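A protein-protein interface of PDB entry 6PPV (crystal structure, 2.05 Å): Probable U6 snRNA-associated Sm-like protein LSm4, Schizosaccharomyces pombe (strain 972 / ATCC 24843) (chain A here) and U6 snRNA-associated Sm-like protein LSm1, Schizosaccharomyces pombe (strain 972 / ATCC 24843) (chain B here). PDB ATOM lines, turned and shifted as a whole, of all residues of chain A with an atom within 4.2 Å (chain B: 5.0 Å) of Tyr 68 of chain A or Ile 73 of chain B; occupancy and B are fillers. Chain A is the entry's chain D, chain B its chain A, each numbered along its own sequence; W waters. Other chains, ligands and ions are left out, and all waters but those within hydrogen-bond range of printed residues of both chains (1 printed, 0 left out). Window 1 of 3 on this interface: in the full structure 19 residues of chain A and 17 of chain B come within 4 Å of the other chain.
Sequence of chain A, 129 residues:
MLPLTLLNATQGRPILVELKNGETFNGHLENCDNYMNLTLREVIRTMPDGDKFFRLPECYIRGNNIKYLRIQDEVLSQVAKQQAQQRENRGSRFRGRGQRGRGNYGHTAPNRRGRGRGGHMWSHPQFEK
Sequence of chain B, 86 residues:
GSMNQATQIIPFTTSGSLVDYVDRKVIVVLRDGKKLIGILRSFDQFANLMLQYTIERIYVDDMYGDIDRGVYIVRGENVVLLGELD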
ATOM      1  N   PRO A   3      -7.886 -14.378  12.846  1.00  0.00           N
ATOM      2  CA  PRO A   3      -6.628 -14.853  13.457  1.00  0.00           C
ATOM      3  C   PRO A   3      -6.623 -16.333  13.815  1.00  0.00           C
ATOM      4  O   PRO A   3      -5.662 -17.045  13.496  1.00  0.00           O
ATOM      5  CB  PRO A   3      -6.511 -13.966  14.705  1.00  0.00           C
ATOM      6  CG  PRO A   3      -7.224 -12.690  14.326  1.00  0.00           C
ATOM      7  CD  PRO A   3      -8.378 -13.131  13.467  1.00  0.00           C
ATOM      8  N   LEU A   6      -6.423 -18.595  10.731  1.00  0.00           N
ATOM      9  CA  LEU A   6      -5.024 -18.705  10.331  1.00  0.00           C
ATOM     10  C   LEU A   6      -4.270 -19.682  11.226  1.00  0.00           C
ATOM     11  O   LEU A   6      -3.506 -20.530  10.742  1.00  0.00           O
ATOM     12  CB  LEU A   6      -4.365 -17.324  10.372  1.00  0.00           C
ATOM     13  CG  LEU A   6      -2.881 -17.310  10.037  1.00  0.00           C
ATOM     14  CD1 LEU A   6      -2.668 -17.857   8.625  1.00  0.00           C
ATOM     15  CD2 LEU A   6      -2.306 -15.902  10.174  1.00  0.00           C
ATOM     16  N   LEU A   7      -4.491 -19.582  12.542  1.00  0.00           N
ATOM     17  CA  LEU A   7      -3.820 -20.466  13.487  1.00  0.00           C
ATOM     18  C   LEU A   7      -4.140 -21.934  13.197  1.00  0.00           C
ATOM     19  O   LEU A   7      -3.239 -22.777  13.131  1.00  0.00           O
ATOM     20  CB  LEU A   7      -4.223 -20.088  14.915  1.00  0.00           C
ATOM     21  CG  LEU A   7      -3.701 -21.042  15.981  1.00  0.00           C
ATOM     22  CD1 LEU A   7      -2.182 -21.047  15.954  1.00  0.00           C
ATOM     23  CD2 LEU A   7      -4.226 -20.684  17.365  1.00  0.00           C
ATOM     24  N   LEU A  16       6.467 -19.808  15.993  1.00  0.00           N
ATOM     25  CA  LEU A  16       7.141 -19.287  17.171  1.00  0.00           C
ATOM     26  C   LEU A  16       6.076 -18.800  18.140  1.00  0.00           C
ATOM     27  O   LEU A  16       5.210 -18.008  17.764  1.00  0.00           O
ATOM     28  CB  LEU A  16       8.116 -18.153  16.813  1.00  0.00           C
ATOM     29  CG  LEU A  16       8.959 -17.468  17.909  1.00  0.00           C
ATOM     30  CD1 LEU A  16      10.134 -16.709  17.295  1.00  0.00           C
ATOM     31  CD2 LEU A  16       8.158 -16.492  18.770  1.00  0.00           C
ATOM     32  N   VAL A  17       6.144 -19.262  19.383  1.00  0.00           N
ATOM     33  CA  VAL A  17       5.241 -18.818  20.433  1.00  0.00           C
ATOM     34  C   VAL A  17       6.053 -18.035  21.451  1.00  0.00           C
ATOM     35  O   VAL A  17       7.041 -18.548  21.984  1.00  0.00           O
ATOM     36  CB  VAL A  17       4.538 -20.005  21.112  1.00  0.00           C
ATOM     37  CG1 VAL A  17       3.460 -19.508  22.084  1.00  0.00           C
ATOM     38  CG2 VAL A  17       3.958 -20.927  20.084  1.00  0.00           C
ATOM     39  N   GLU A  18       5.639 -16.806  21.743  1.00  0.00           N
ATOM     40  CA  GLU A  18       6.174 -16.106  22.898  1.00  0.00           C
ATOM     41  C   GLU A  18       5.127 -16.053  24.001  1.00  0.00           C
ATOM     42  O   GLU A  18       3.996 -15.593  23.774  1.00  0.00           O
ATOM     43  CB  GLU A  18       6.657 -14.696  22.560  1.00  0.00           C
ATOM     44  CG  GLU A  18       7.415 -14.094  23.759  1.00  0.00           C
ATOM     45  CD  GLU A  18       8.183 -12.815  23.431  1.00  0.00           C
ATOM     46  OE1 GLU A  18       8.234 -11.916  24.301  1.00  0.00           O
ATOM     47  OE2 GLU A  18       8.739 -12.711  22.314  1.00  0.00           O
ATOM     48  N   ILE A  66      -0.126 -17.028  26.496  1.00  0.00           N
ATOM     49  CA  ILE A  66       0.536 -16.593  25.264  1.00  0.00           C
ATOM     50  C   ILE A  66       0.548 -15.069  25.171  1.00  0.00           C
ATOM     51  O   ILE A  66      -0.454 -14.396  25.450  1.00  0.00           O
ATOM     52  CB  ILE A  66      -0.147 -17.226  24.036  1.00  0.00           C
ATOM     53  CG1 ILE A  66       0.124 -18.738  24.004  1.00  0.00           C
ATOM     54  CG2 ILE A  66       0.319 -16.559  22.719  1.00  0.00           C
ATOM     55  CD1 ILE A  66      -0.755 -19.490  23.015  1.00  0.00           C
ATOM     56  N   LYS A  67       1.705 -14.521  24.798  1.00  0.00           N
ATOM     57  CA  LYS A  67       1.822 -13.133  24.364  1.00  0.00           C
ATOM     58  C   LYS A  67       1.536 -13.000  22.865  1.00  0.00           C
ATOM     59  O   LYS A  67       0.602 -12.299  22.462  1.00  0.00           O
ATOM     60  CB  LYS A  67       3.218 -12.593  24.699  1.00  0.00           C
ATOM     61  CG  LYS A  67       3.442 -11.137  24.261  1.00  0.00           C
ATOM     62  CD  LYS A  67       4.882 -10.690  24.512  1.00  0.00           C
ATOM     63  CE  LYS A  67       5.282 -10.925  25.970  1.00  0.00           C
ATOM     64  NZ  LYS A  67       6.688 -10.515  26.217  1.00  0.00           N
ATOM     65  N   TYR A  68       2.313 -13.686  22.029  1.00  0.00           N
ATOM     66  CA  TYR A  68       1.977 -13.680  20.607  1.00  0.00           C
ATOM     67  C   TYR A  68       2.531 -14.915  19.921  1.00  0.00           C
ATOM     68  O   TYR A  68       3.257 -15.720  20.506  1.00  0.00           O
ATOM     69  CB  TYR A  68       2.478 -12.415  19.877  1.00  0.00           C
ATOM     70  CG  TYR A  68       3.951 -12.140  20.042  1.00  0.00           C
ATOM     71  CD1 TYR A  68       4.908 -12.931  19.410  1.00  0.00           C
ATOM     72  CD2 TYR A  68       4.393 -11.090  20.832  1.00  0.00           C
ATOM     73  CE1 TYR A  68       6.264 -12.693  19.577  1.00  0.00           C
ATOM     74  CE2 TYR A  68       5.745 -10.846  21.003  1.00  0.00           C
ATOM     75  CZ  TYR A  68       6.669 -11.650  20.373  1.00  0.00           C
ATOM     76  OH  TYR A  68       8.009 -11.408  20.535  1.00  0.00           O
ATOM     77  N   LEU A  69       2.178 -15.029  18.649  1.00  0.00           N
ATOM     78  CA  LEU A  69       2.613 -16.093  17.766  1.00  0.00           C
ATOM     79  C   LEU A  69       3.158 -15.453  16.502  1.00  0.00           C
ATOM     80  O   LEU A  69       2.628 -14.439  16.033  1.00  0.00           O
ATOM     81  CB  LEU A  69       1.451 -17.033  17.408  1.00  0.00           C
ATOM     82  CG  LEU A  69       0.704 -17.651  18.586  1.00  0.00           C
ATOM     83  CD1 LEU A  69      -0.769 -17.783  18.288  1.00  0.00           C
ATOM     84  CD2 LEU A  69       1.275 -19.010  18.862  1.00  0.00           C
ATOM     85  N   LEU B  30       2.049  -3.286  22.934  1.00  0.00           N
ATOM     86  CA  LEU B  30       1.774  -4.434  23.781  1.00  0.00           C
ATOM     87  C   LEU B  30       2.023  -4.096  25.246  1.00  0.00           C
ATOM     88  O   LEU B  30       2.720  -3.136  25.575  1.00  0.00           O
ATOM     89  CB  LEU B  30       2.647  -5.631  23.379  1.00  0.00           C
ATOM     90  CG  LEU B  30       2.560  -6.104  21.918  1.00  0.00           C
ATOM     91  CD1 LEU B  30       3.273  -7.439  21.758  1.00  0.00           C
ATOM     92  CD2 LEU B  30       1.113  -6.220  21.469  1.00  0.00           C
ATOM     93  N   LYS B  34       6.388  -3.578  23.841  1.00  0.00           N
ATOM     94  CA  LYS B  34       6.863  -3.705  22.467  1.00  0.00           C
ATOM     95  C   LYS B  34       6.027  -2.876  21.502  1.00  0.00           C
ATOM     96  O   LYS B  34       4.812  -2.726  21.662  1.00  0.00           O
ATOM     97  CB  LYS B  34       6.838  -5.163  22.005  1.00  0.00           C
ATOM     98  CG  LYS B  34       7.952  -6.024  22.540  1.00  0.00           C
ATOM     99  CD  LYS B  34       7.841  -7.440  21.963  1.00  0.00           C
ATOM    100  CE  LYS B  34       9.127  -8.221  22.143  1.00  0.00           C
ATOM    101  NZ  LYS B  34       9.302  -8.724  23.530  1.00  0.00           N
ATOM    102  N   LEU B  49      -5.254 -10.019  17.100  1.00  0.00           N
ATOM    103  CA  LEU B  49      -4.875  -9.315  15.883  1.00  0.00           C
ATOM    104  C   LEU B  49      -4.059 -10.231  14.984  1.00  0.00           C
ATOM    105  O   LEU B  49      -3.330 -11.104  15.457  1.00  0.00           O
ATOM    106  CB  LEU B  49      -4.054  -8.061  16.195  1.00  0.00           C
ATOM    107  CG  LEU B  49      -4.659  -7.042  17.155  1.00  0.00           C
ATOM    108  CD1 LEU B  49      -3.679  -5.883  17.392  1.00  0.00           C
ATOM    109  CD2 LEU B  49      -5.980  -6.539  16.617  1.00  0.00           C
ATOM    110  N   MET B  50      -4.165 -10.013  13.681  1.00  0.00           N
ATOM    111  CA  MET B  50      -3.281 -10.664  12.729  1.00  0.00           C
ATOM    112  C   MET B  50      -2.689  -9.588  11.838  1.00  0.00           C
ATOM    113  O   MET B  50      -3.436  -8.879  11.140  1.00  0.00           O
ATOM    114  CB  MET B  50      -4.000 -11.732  11.903  1.00  0.00           C
ATOM    115  CG  MET B  50      -3.021 -12.616  11.149  1.00  0.00           C
ATOM    116  SD  MET B  50      -2.653 -12.072   9.466  1.00  0.00           S
ATOM    117  CE  MET B  50      -4.046 -12.797   8.601  1.00  0.00           C
ATOM    118  N   GLU B  56       9.354  -5.039  14.251  1.00  0.00           N
ATOM    119  CA  GLU B  56       9.409  -4.660  15.652  1.00  0.00           C
ATOM    120  C   GLU B  56      10.369  -3.482  15.762  1.00  0.00           C
ATOM    121  O   GLU B  56      11.522  -3.572  15.320  1.00  0.00           O
ATOM    122  CB  GLU B  56       9.861  -5.827  16.525  1.00  0.00           C
ATOM    123  CG  GLU B  56       9.731  -5.562  18.014  1.00  0.00           C
ATOM    124  CD  GLU B  56      10.305  -6.684  18.853  1.00  0.00           C
ATOM    125  OE1 GLU B  56      10.698  -6.415  20.004  1.00  0.00           O
ATOM    126  OE2 GLU B  56      10.378  -7.835  18.359  1.00  0.00           O
ATOM    127  N   VAL B  71       4.716 -12.339  10.039  1.00  0.00           N
ATOM    128  CA  VAL B  71       3.308 -12.358  10.404  1.00  0.00           C
ATOM    129  C   VAL B  71       3.204 -12.585  11.907  1.00  0.00           C
ATOM    130  O   VAL B  71       3.893 -13.454  12.458  1.00  0.00           O
ATOM    131  CB  VAL B  71       2.560 -13.451   9.623  1.00  0.00           C
ATOM    132  CG1 VAL B  71       1.140 -13.618  10.150  1.00  0.00           C
ATOM    133  CG2 VAL B  71       2.565 -13.133   8.116  1.00  0.00           C
ATOM    134  N   TYR B  72       2.352 -11.804  12.572  1.00  0.00           N
ATOM    135  CA  TYR B  72       2.002 -12.024  13.974  1.00  0.00           C
ATOM    136  C   TYR B  72       0.528 -12.374  14.109  1.00  0.00           C
ATOM    137  O   TYR B  72      -0.321 -11.797  13.417  1.00  0.00           O
ATOM    138  CB  TYR B  72       2.228 -10.788  14.847  1.00  0.00           C
ATOM    139  CG  TYR B  72       3.640 -10.461  15.233  1.00  0.00           C
ATOM    140  CD1 TYR B  72       4.427  -9.675  14.414  1.00  0.00           C
ATOM    141  CD2 TYR B  72       4.163 -10.878  16.449  1.00  0.00           C
ATOM    142  CE1 TYR B  72       5.707  -9.339  14.772  1.00  0.00           C
ATOM    143  CE2 TYR B  72       5.447 -10.550  16.818  1.00  0.00           C
ATOM    144  CZ  TYR B  72       6.216  -9.775  15.969  1.00  0.00           C
ATOM    145  OH  TYR B  72       7.499  -9.431  16.314  1.00  0.00           O
ATOM    146  N   ILE B  73       0.237 -13.290  15.033  1.00  0.00           N
ATOM    147  CA  ILE B  73      -1.057 -13.385  15.692  1.00  0.00           C
ATOM    148  C   ILE B  73      -0.834 -12.904  17.122  1.00  0.00           C
ATOM    149  O   ILE B  73      -0.153 -13.580  17.907  1.00  0.00           O
ATOM    150  CB  ILE B  73      -1.626 -14.811  15.669  1.00  0.00           C
ATOM    151  CG1 ILE B  73      -1.956 -15.251  14.244  1.00  0.00           C
ATOM    152  CG2 ILE B  73      -2.861 -14.897  16.527  1.00  0.00           C
ATOM    153  CD1 ILE B  73      -2.453 -16.703  14.155  1.00  0.00           C
ATOM    154  N   VAL B  74      -1.369 -11.721  17.455  1.00  0.00           N
ATOM    155  CA  VAL B  74      -1.247 -11.152  18.795  1.00  0.00           C
ATOM    156  C   VAL B  74      -2.491 -11.499  19.599  1.00  0.00           C
ATOM    157  O   VAL B  74      -3.618 -11.218  19.171  1.00  0.00           O
ATOM    158  CB  VAL B  74      -1.035  -9.629  18.752  1.00  0.00           C
ATOM    159  CG1 VAL B  74      -0.773  -9.107  20.159  1.00  0.00           C
ATOM    160  CG2 VAL B  74       0.114  -9.258  17.823  1.00  0.00           C
ATOM    161  N   ARG B  75      -2.294 -12.107  20.766  1.00  0.00           N
ATOM    162  CA  ARG B  75      -3.422 -12.376  21.654  1.00  0.00           C
ATOM    163  C   ARG B  75      -3.959 -11.061  22.217  1.00  0.00           C
ATOM    164  O   ARG B  75      -3.197 -10.240  22.734  1.00  0.00           O
ATOM    165  CB  ARG B  75      -3.002 -13.323  22.774  1.00  0.00           C
ATOM    166  CG  ARG B  75      -4.145 -14.000  23.490  1.00  0.00           C
ATOM    167  CD  ARG B  75      -3.624 -14.833  24.635  1.00  0.00           C
ATOM    168  NE  ARG B  75      -4.647 -15.055  25.650  1.00  0.00           N
ATOM    169  CZ  ARG B  75      -5.623 -15.956  25.552  1.00  0.00           C
ATOM    170  NH1 ARG B  75      -5.721 -16.733  24.484  1.00  0.00           N
ATOM    171  NH2 ARG B  75      -6.505 -16.079  26.533  1.00  0.00           N
HETATM  172  O   HOH W   1       8.784 -10.077  18.368  1.00  0.00           O
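NZ of Lys 34 of chain B is in salt-bridge range of OE1 of Glu 18 of chain A (3.5 Å). The backbone carbonyl oxygen of Lys 67 of chain A lies within hydrogen-bond range of the backbone NH of Arg 75 of chain B, at 3.4 Å. O of Leu 69 of chain A is in hydrogen-bond range of N of Ile 73 of chain B, at 2.8 Å.
Of chain B, only Leu 30 (3.9 Å), Lys 34 (3.7 Å), Tyr 72 (3.6 Å) and Ile 73 (3.4 Å) come within 4 Å of Tyr 68 of chain A. Ile 73 of chain B touches just these residues of chain A: Pro 3 (3.3 Å), Leu 7 (3.9 Å), Tyr 68 (3.4 Å) and Leu 69 (2.8 Å). Of the printed residues of chain A, Tyr 72 of chain B touches Tyr 68 (3.6 Å) and Leu 69 (3.2 Å). Of the printed residues of chain A, Val 71 of chain B touches Leu 69. Printed residues of chain B within 4 Å of Lys 67 of chain A: Arg 75. Val 74 of chain B touches none of the printed residues of chain A. Leu 49 of chain B touches none of the printed residues of chain A. The nearest residue of chain A that does not touch Ile 73 of chain B is Leu 6 of chain A (4.1 Å).
Printed residues of chain B that touch a printed residue of chain A: Leu 30, Lys 34, Met 50, Val 71, Tyr 72, Ile 73 and Arg 75. Hydrophobic or aromatic side chains of chain B within 4 Å of the printed part of chain A: Leu 30, Met 50, Tyr 72 and Ile 73. Along chain B the printed residues that touch a printed residue of chain A span positions 30 to 75. Printed residues of chain A that touch a printed residue of chain B: Pro 3, Leu 6, Leu 7, Glu 18, Ile 66, Lys 67, Tyr 68 and Leu 69. Hydrophobic or aromatic side chains of chain A within 4 Å of the printed part of chain B: Leu 6, Leu 7, Tyr 68 and Leu 69.
The backbone carbonyl oxygen of Tyr 68 of chain A sits at hydrogen-bond distance from the backbone NH of Glu 18 of chain A (2.9 Å). The side-chain carboxylate (OE1) of Glu 18 of chain A is in salt-bridge range of the side-chain amino group (NZ) of Lys 67 of chain A (2.8 Å).
Among the printed residues, pairs that only touch across the chains: Pro 3 of chain A with Ile 73 of chain B, Leu 6 of chain A with Met 50 of chain B, Leu 7 of chain A with Ile 73 of chain B, Ile 66 of chain A with Arg 75 of chain B, Tyr 68 of chain A with Leu 30 of chain B, Tyr 68 of chain A with Lys 34 of chain B, Tyr 68 of chain A with Tyr 72 of chain B, Tyr 68 of chain A with Ile 73 of chain B, Leu 69 of chain A with Val 71 of chain B and Leu 69 of chain A with Tyr 72 of chain B.
Water W1 lies within hydrogen-bond range of the side-chain hydroxyl of Tyr 72 of chain B (2.5 Å), the side-chain hydroxyl of Tyr 68 of chain A (2.7 Å) and the side-chain carboxylate of Glu 56 of chain B (2.8 Å).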
